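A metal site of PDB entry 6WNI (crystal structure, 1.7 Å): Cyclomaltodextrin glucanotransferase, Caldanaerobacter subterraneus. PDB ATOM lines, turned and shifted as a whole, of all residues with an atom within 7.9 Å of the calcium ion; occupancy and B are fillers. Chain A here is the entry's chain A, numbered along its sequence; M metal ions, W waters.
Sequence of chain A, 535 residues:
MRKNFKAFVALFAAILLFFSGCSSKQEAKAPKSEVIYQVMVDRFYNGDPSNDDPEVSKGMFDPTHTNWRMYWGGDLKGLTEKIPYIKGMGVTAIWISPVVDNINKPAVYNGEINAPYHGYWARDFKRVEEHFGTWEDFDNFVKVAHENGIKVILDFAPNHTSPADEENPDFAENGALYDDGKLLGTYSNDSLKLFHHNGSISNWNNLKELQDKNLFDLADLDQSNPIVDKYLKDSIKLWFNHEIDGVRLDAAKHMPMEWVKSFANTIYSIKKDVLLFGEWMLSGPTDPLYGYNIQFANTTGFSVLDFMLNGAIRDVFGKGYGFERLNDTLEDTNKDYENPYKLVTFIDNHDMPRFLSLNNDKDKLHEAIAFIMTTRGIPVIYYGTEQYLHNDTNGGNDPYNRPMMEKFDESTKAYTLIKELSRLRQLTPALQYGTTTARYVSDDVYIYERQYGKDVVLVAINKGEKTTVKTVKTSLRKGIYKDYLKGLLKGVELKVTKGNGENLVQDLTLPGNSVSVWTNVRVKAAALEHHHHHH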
ATOM      1  N   VAL A  41      29.394 -18.719  21.894  1.00  0.00           N
ATOM      2  CA  VAL A  41      28.074 -18.830  21.266  1.00  0.00           C
ATOM      3  C   VAL A  41      27.387 -20.137  21.591  1.00  0.00           C
ATOM      4  O   VAL A  41      26.198 -20.168  21.952  1.00  0.00           O
ATOM      5  CB  VAL A  41      28.200 -18.648  19.742  1.00  0.00           C
ATOM      6  CG1 VAL A  41      26.827 -18.811  19.076  1.00  0.00           C
ATOM      7  CG2 VAL A  41      28.718 -17.263  19.429  1.00  0.00           C
ATOM      8  N   ASP A  42      28.113 -21.248  21.474  1.00  0.00           N
ATOM      9  CA  ASP A  42      27.486 -22.556  21.679  1.00  0.00           C
ATOM     10  C   ASP A  42      26.971 -22.735  23.101  1.00  0.00           C
ATOM     11  O   ASP A  42      26.083 -23.558  23.322  1.00  0.00           O
ATOM     12  CB  ASP A  42      28.472 -23.680  21.349  1.00  0.00           C
ATOM     13  CG  ASP A  42      27.866 -25.060  21.566  1.00  0.00           C
ATOM     14  OD1 ASP A  42      26.948 -25.416  20.808  1.00  0.00           O
ATOM     15  OD2 ASP A  42      28.302 -25.790  22.508  1.00  0.00           O
ATOM     16  N   TYR A  45      22.920 -19.234  24.475  1.00  0.00           N
ATOM     17  CA  TYR A  45      21.483 -19.446  24.404  1.00  0.00           C
ATOM     18  C   TYR A  45      21.107 -20.147  23.097  1.00  0.00           C
ATOM     19  O   TYR A  45      21.439 -19.678  22.004  1.00  0.00           O
ATOM     20  CB  TYR A  45      20.720 -18.122  24.529  1.00  0.00           C
ATOM     21  CG  TYR A  45      19.251 -18.307  24.827  1.00  0.00           C
ATOM     22  CD1 TYR A  45      18.837 -18.928  26.001  1.00  0.00           C
ATOM     23  CD2 TYR A  45      18.284 -17.836  23.953  1.00  0.00           C
ATOM     24  CE1 TYR A  45      17.497 -19.096  26.269  1.00  0.00           C
ATOM     25  CE2 TYR A  45      16.932 -17.997  24.220  1.00  0.00           C
ATOM     26  CZ  TYR A  45      16.547 -18.625  25.391  1.00  0.00           C
ATOM     27  OH  TYR A  45      15.214 -18.780  25.668  1.00  0.00           O
ATOM     28  N   ASN A  46      20.382 -21.246  23.228  1.00  0.00           N
ATOM     29  CA  ASN A  46      19.928 -22.013  22.065  1.00  0.00           C
ATOM     30  C   ASN A  46      18.573 -21.463  21.633  1.00  0.00           C
ATOM     31  O   ASN A  46      17.539 -21.807  22.211  1.00  0.00           O
ATOM     32  CB  ASN A  46      19.855 -23.494  22.425  1.00  0.00           C
ATOM     33  CG  ASN A  46      19.463 -24.353  21.244  1.00  0.00           C
ATOM     34  OD1 ASN A  46      19.196 -23.856  20.154  1.00  0.00           O
ATOM     35  ND2 ASN A  46      19.455 -25.667  21.457  1.00  0.00           N
ATOM     36  N   GLY A  47      18.566 -20.614  20.608  1.00  0.00           N
ATOM     37  CA  GLY A  47      17.318 -20.076  20.092  1.00  0.00           C
ATOM     38  C   GLY A  47      16.669 -20.869  18.983  1.00  0.00           C
ATOM     39  O   GLY A  47      15.505 -20.632  18.644  1.00  0.00           O
ATOM     40  N   ASP A  48      17.387 -21.813  18.420  1.00  0.00           N
ATOM     41  CA  ASP A  48      16.885 -22.537  17.254  1.00  0.00           C
ATOM     42  C   ASP A  48      17.279 -23.998  17.349  1.00  0.00           C
ATOM     43  O   ASP A  48      18.465 -24.331  17.233  1.00  0.00           O
ATOM     44  CB  ASP A  48      17.430 -21.910  15.961  1.00  0.00           C
ATOM     45  CG  ASP A  48      16.834 -22.516  14.706  1.00  0.00           C
ATOM     46  OD1 ASP A  48      15.990 -23.446  14.810  1.00  0.00           O
ATOM     47  OD2 ASP A  48      17.193 -22.059  13.599  1.00  0.00           O
ATOM     48  N   PRO A  49      16.338 -24.902  17.600  1.00  0.00           N
ATOM     49  CA  PRO A  49      16.699 -26.325  17.676  1.00  0.00           C
ATOM     50  C   PRO A  49      17.007 -26.949  16.321  1.00  0.00           C
ATOM     51  O   PRO A  49      17.613 -28.027  16.290  1.00  0.00           O
ATOM     52  CB  PRO A  49      15.464 -26.960  18.324  1.00  0.00           C
ATOM     53  CG  PRO A  49      14.340 -26.064  17.958  1.00  0.00           C
ATOM     54  CD  PRO A  49      14.895 -24.678  17.810  1.00  0.00           C
ATOM     55  N   SER A  50      16.642 -26.301  15.222  1.00  0.00           N
ATOM     56  CA  SER A  50      16.830 -26.922  13.919  1.00  0.00           C
ATOM     57  C   SER A  50      18.292 -26.919  13.474  1.00  0.00           C
ATOM     58  O   SER A  50      18.638 -27.676  12.568  1.00  0.00           O
ATOM     59  CB  SER A  50      15.963 -26.218  12.870  1.00  0.00           C
ATOM     60  OG  SER A  50      16.264 -24.839  12.810  1.00  0.00           O
ATOM     61  N   ASN A  51      19.149 -26.112  14.094  1.00  0.00           N
ATOM     62  CA  ASN A  51      20.573 -26.129  13.758  1.00  0.00           C
ATOM     63  C   ASN A  51      21.423 -26.820  14.811  1.00  0.00           C
ATOM     64  O   ASN A  51      22.667 -26.771  14.714  1.00  0.00           O
ATOM     65  CB  ASN A  51      21.083 -24.693  13.503  1.00  0.00           C
ATOM     66  CG  ASN A  51      20.900 -23.766  14.696  1.00  0.00           C
ATOM     67  OD1 ASN A  51      20.806 -24.222  15.833  1.00  0.00           O
ATOM     68  ND2 ASN A  51      20.859 -22.459  14.432  1.00  0.00           N
ATOM     69  N   ASP A  52      20.811 -27.460  15.810  1.00  0.00           N
ATOM     70  CA  ASP A  52      21.565 -28.162  16.846  1.00  0.00           C
ATOM     71  C   ASP A  52      22.407 -29.274  16.248  1.00  0.00           C
ATOM     72  O   ASP A  52      23.545 -29.500  16.672  1.00  0.00           O
ATOM     73  CB  ASP A  52      20.621 -28.755  17.892  1.00  0.00           C
ATOM     74  CG  ASP A  52      20.000 -27.717  18.788  1.00  0.00           C
ATOM     75  OD1 ASP A  52      20.331 -26.519  18.629  1.00  0.00           O
ATOM     76  OD2 ASP A  52      19.192 -28.099  19.662  1.00  0.00           O
ATOM     77  N   ASP A  53      21.864 -29.999  15.270  1.00  0.00           N
ATOM     78  CA  ASP A  53      22.505 -31.210  14.751  1.00  0.00           C
ATOM     79  C   ASP A  53      22.329 -31.220  13.239  1.00  0.00           C
ATOM     80  O   ASP A  53      21.525 -31.985  12.686  1.00  0.00           O
ATOM     81  CB  ASP A  53      21.896 -32.451  15.408  1.00  0.00           C
ATOM     82  CG  ASP A  53      22.790 -33.662  15.336  1.00  0.00           C
ATOM     83  OD1 ASP A  53      23.973 -33.563  14.946  1.00  0.00           O
ATOM     84  OD2 ASP A  53      22.289 -34.741  15.699  1.00  0.00           O
ATOM     85  N   PHE A  61      26.372 -33.219  18.521  1.00  0.00           N
ATOM     86  CA  PHE A  61      25.492 -32.468  19.401  1.00  0.00           C
ATOM     87  C   PHE A  61      25.063 -33.345  20.571  1.00  0.00           C
ATOM     88  O   PHE A  61      24.625 -34.479  20.385  1.00  0.00           O
ATOM     89  CB  PHE A  61      24.274 -31.986  18.629  1.00  0.00           C
ATOM     90  CG  PHE A  61      23.167 -31.474  19.498  1.00  0.00           C
ATOM     91  CD1 PHE A  61      23.329 -30.327  20.259  1.00  0.00           C
ATOM     92  CD2 PHE A  61      21.936 -32.120  19.532  1.00  0.00           C
ATOM     93  CE1 PHE A  61      22.295 -29.842  21.048  1.00  0.00           C
ATOM     94  CE2 PHE A  61      20.902 -31.649  20.319  1.00  0.00           C
ATOM     95  CZ  PHE A  61      21.082 -30.503  21.077  1.00  0.00           C
ATOM     96  N   TRP A  72      26.510 -27.934  22.365  1.00  0.00           N
ATOM     97  CA  TRP A  72      25.346 -27.921  23.241  1.00  0.00           C
ATOM     98  C   TRP A  72      24.157 -27.158  22.679  1.00  0.00           C
ATOM     99  O   TRP A  72      23.052 -27.270  23.232  1.00  0.00           O
ATOM    100  CB  TRP A  72      25.736 -27.349  24.619  1.00  0.00           C
ATOM    101  CG  TRP A  72      26.525 -28.347  25.449  1.00  0.00           C
ATOM    102  CD1 TRP A  72      26.948 -29.586  25.052  1.00  0.00           C
ATOM    103  CD2 TRP A  72      26.941 -28.195  26.816  1.00  0.00           C
ATOM    104  NE1 TRP A  72      27.610 -30.207  26.078  1.00  0.00           N
ATOM    105  CE2 TRP A  72      27.633 -29.378  27.174  1.00  0.00           C
ATOM    106  CE3 TRP A  72      26.811 -27.175  27.764  1.00  0.00           C
ATOM    107  CZ2 TRP A  72      28.195 -29.572  28.447  1.00  0.00           C
ATOM    108  CZ3 TRP A  72      27.366 -27.368  29.030  1.00  0.00           C
ATOM    109  CH2 TRP A  72      28.041 -28.568  29.359  1.00  0.00           C
ATOM    110  N   GLY A  73      24.332 -26.401  21.584  1.00  0.00           N
ATOM    111  CA  GLY A  73      23.216 -25.872  20.828  1.00  0.00           C
ATOM    112  C   GLY A  73      23.045 -24.360  20.827  1.00  0.00           C
ATOM    113  O   GLY A  73      22.151 -23.868  20.126  1.00  0.00           O
ATOM    114  N   GLY A  74      23.836 -23.599  21.596  1.00  0.00           N
ATOM    115  CA  GLY A  74      23.735 -22.154  21.556  1.00  0.00           C
ATOM    116  C   GLY A  74      24.016 -21.619  20.164  1.00  0.00           C
ATOM    117  O   GLY A  74      24.811 -22.178  19.411  1.00  0.00           O
ATOM    118  N   ASP A  75      23.345 -20.528  19.786  1.00  0.00           N
ATOM    119  CA  ASP A  75      23.411 -20.112  18.398  1.00  0.00           C
ATOM    120  C   ASP A  75      23.183 -18.615  18.281  1.00  0.00           C
ATOM    121  O   ASP A  75      23.012 -17.899  19.274  1.00  0.00           O
ATOM    122  CB  ASP A  75      22.407 -20.892  17.558  1.00  0.00           C
ATOM    123  CG  ASP A  75      21.006 -20.908  18.170  1.00  0.00           C
ATOM    124  OD1 ASP A  75      20.561 -19.887  18.721  1.00  0.00           O
ATOM    125  OD2 ASP A  75      20.361 -21.956  18.109  1.00  0.00           O
ATOM    126  N   LEU A  76      23.209 -18.137  17.029  1.00  0.00           N
ATOM    127  CA  LEU A  76      23.122 -16.697  16.786  1.00  0.00           C
ATOM    128  C   LEU A  76      21.725 -16.183  17.072  1.00  0.00           C
ATOM    129  O   LEU A  76      21.572 -15.093  17.619  1.00  0.00           O
ATOM    130  CB  LEU A  76      23.544 -16.386  15.347  1.00  0.00           C
ATOM    131  CG  LEU A  76      25.055 -16.517  15.124  1.00  0.00           C
ATOM    132  CD1 LEU A  76      25.361 -16.647  13.632  1.00  0.00           C
ATOM    133  CD2 LEU A  76      25.807 -15.338  15.741  1.00  0.00           C
ATOM    134  N   LYS A  77      20.704 -16.963  16.712  1.00  0.00           N
ATOM    135  CA  LYS A  77      19.342 -16.523  17.025  1.00  0.00           C
ATOM    136  C   LYS A  77      19.155 -16.374  18.526  1.00  0.00           C
ATOM    137  O   LYS A  77      18.566 -15.384  18.991  1.00  0.00           O
ATOM    138  CB  LYS A  77      18.317 -17.504  16.441  1.00  0.00           C
ATOM    139  CG  LYS A  77      16.873 -17.125  16.787  1.00  0.00           C
ATOM    140  CD  LYS A  77      15.855 -18.142  16.264  1.00  0.00           C
ATOM    141  CE  LYS A  77      15.304 -17.710  14.909  1.00  0.00           C
ATOM    142  NZ  LYS A  77      16.333 -17.784  13.834  1.00  0.00           N
ATOM    143  N   GLY A  78      19.668 -17.341  19.299  1.00  0.00           N
ATOM    144  CA  GLY A  78      19.552 -17.234  20.735  1.00  0.00           C
ATOM    145  C   GLY A  78      20.286 -16.026  21.289  1.00  0.00           C
ATOM    146  O   GLY A  78      19.778 -15.322  22.169  1.00  0.00           O
ATOM    147  N   GLU A 130      27.317 -23.552  10.529  1.00  0.00           N
ATOM    148  CA  GLU A 130      25.913 -23.911  10.376  1.00  0.00           C
ATOM    149  C   GLU A 130      25.247 -24.298  11.696  1.00  0.00           C
ATOM    150  O   GLU A 130      24.021 -24.234  11.804  1.00  0.00           O
ATOM    151  CB  GLU A 130      25.769 -25.038   9.337  1.00  0.00           C
ATOM    152  CG  GLU A 130      26.300 -26.409   9.735  1.00  0.00           C
ATOM    153  CD  GLU A 130      27.831 -26.509   9.784  1.00  0.00           C
ATOM    154  OE1 GLU A 130      28.504 -25.605   9.261  1.00  0.00           O
ATOM    155  OE2 GLU A 130      28.358 -27.503  10.308  1.00  0.00           O
ATOM    156  N   HIS A 131      26.023 -24.692  12.720  1.00  0.00           N
ATOM    157  CA  HIS A 131      25.405 -24.931  14.053  1.00  0.00           C
ATOM    158  C   HIS A 131      24.890 -23.624  14.656  1.00  0.00           C
ATOM    159  O   HIS A 131      24.027 -23.670  15.473  1.00  0.00           O
ATOM    160  CB  HIS A 131      26.414 -25.577  15.019  1.00  0.00           C
ATOM    161  CG  HIS A 131      26.722 -27.004  14.716  1.00  0.00           C
ATOM    162  ND1 HIS A 131      27.542 -27.410  13.698  1.00  0.00           N
ATOM    163  CD2 HIS A 131      26.310 -28.138  15.300  1.00  0.00           C
ATOM    164  CE1 HIS A 131      27.607 -28.705  13.678  1.00  0.00           C
ATOM    165  NE2 HIS A 131      26.899 -29.166  14.671  1.00  0.00           N
ATOM    166  N   PHE A 132      25.455 -22.485  14.262  1.00  0.00           N
ATOM    167  CA  PHE A 132      25.120 -21.199  14.850  1.00  0.00           C
ATOM    168  C   PHE A 132      24.171 -20.397  14.000  1.00  0.00           C
ATOM    169  O   PHE A 132      23.466 -19.520  14.528  1.00  0.00           O
ATOM    170  CB  PHE A 132      26.388 -20.358  15.092  1.00  0.00           C
ATOM    171  CG  PHE A 132      27.415 -21.025  15.993  1.00  0.00           C
ATOM    172  CD1 PHE A 132      27.056 -22.014  16.902  1.00  0.00           C
ATOM    173  CD2 PHE A 132      28.757 -20.651  15.909  1.00  0.00           C
ATOM    174  CE1 PHE A 132      28.007 -22.627  17.716  1.00  0.00           C
ATOM    175  CE2 PHE A 132      29.723 -21.252  16.738  1.00  0.00           C
ATOM    176  CZ  PHE A 132      29.345 -22.246  17.637  1.00  0.00           C
ATOM    177  N   GLY A 133      24.148 -20.617  12.693  1.00  0.00           N
ATOM    178  CA  GLY A 133      23.164 -19.998  11.828  1.00  0.00           C
ATOM    179  C   GLY A 133      23.698 -19.770  10.421  1.00  0.00           C
ATOM    180  O   GLY A 133      24.724 -20.296  10.027  1.00  0.00           O
HETATM  181 CA    CA M   1      20.621 -24.286  18.215  1.00  0.00          CA
HETATM  182  O   HOH W   1      22.919 -24.907  17.617  1.00  0.00           O
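The calcium ion is bound by OD1 of Asp 52 (2.3 Å), OD2 of Asp 75 (2.3 Å), O of Asp 48 (2.4 Å), OD1 of Asn 51 (2.4 Å), OD1 of Asn 46 (2.4 Å), water W1 (2.5 Å) and O of Gly 73 (2.5 Å).
The backbone NH (N) of Gly 47 lies within hydrogen-bond range of the side-chain carboxylate (OD1) of Asp 75.
The backbone carbonyl oxygen of Tyr 45 is in hydrogen-bond range of the backbone NH of Asp 75, 3.0 Å away.
N of Gly 78 is in hydrogen-bond range of OD1 of Asp 75.
OD1 of Asp 48 lies within hydrogen-bond range of OG of Ser 50 (2.5 Å).
The side-chain amide oxygen (OD1) of Asn 51 lies close to the backbone carbonyl oxygen (O) of His 131, 3.3 Å away.
The side-chain carboxylate (OD1) of Asp 42 is in hydrogen-bond range of the backbone NH (N) of Gly 73, at 2.9 Å.
Within 4 Å of the calcium ion: Asn 46, Asp 48, Asn 51, Asp 52, Gly 73 and Asp 75.
The nearest printed residue that does not touch the calcium ion is Pro 49 (4.4 Å).
Water W1 bridges O of His 131 (2.7 Å) and O of Asn 51 (3.5 Å).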
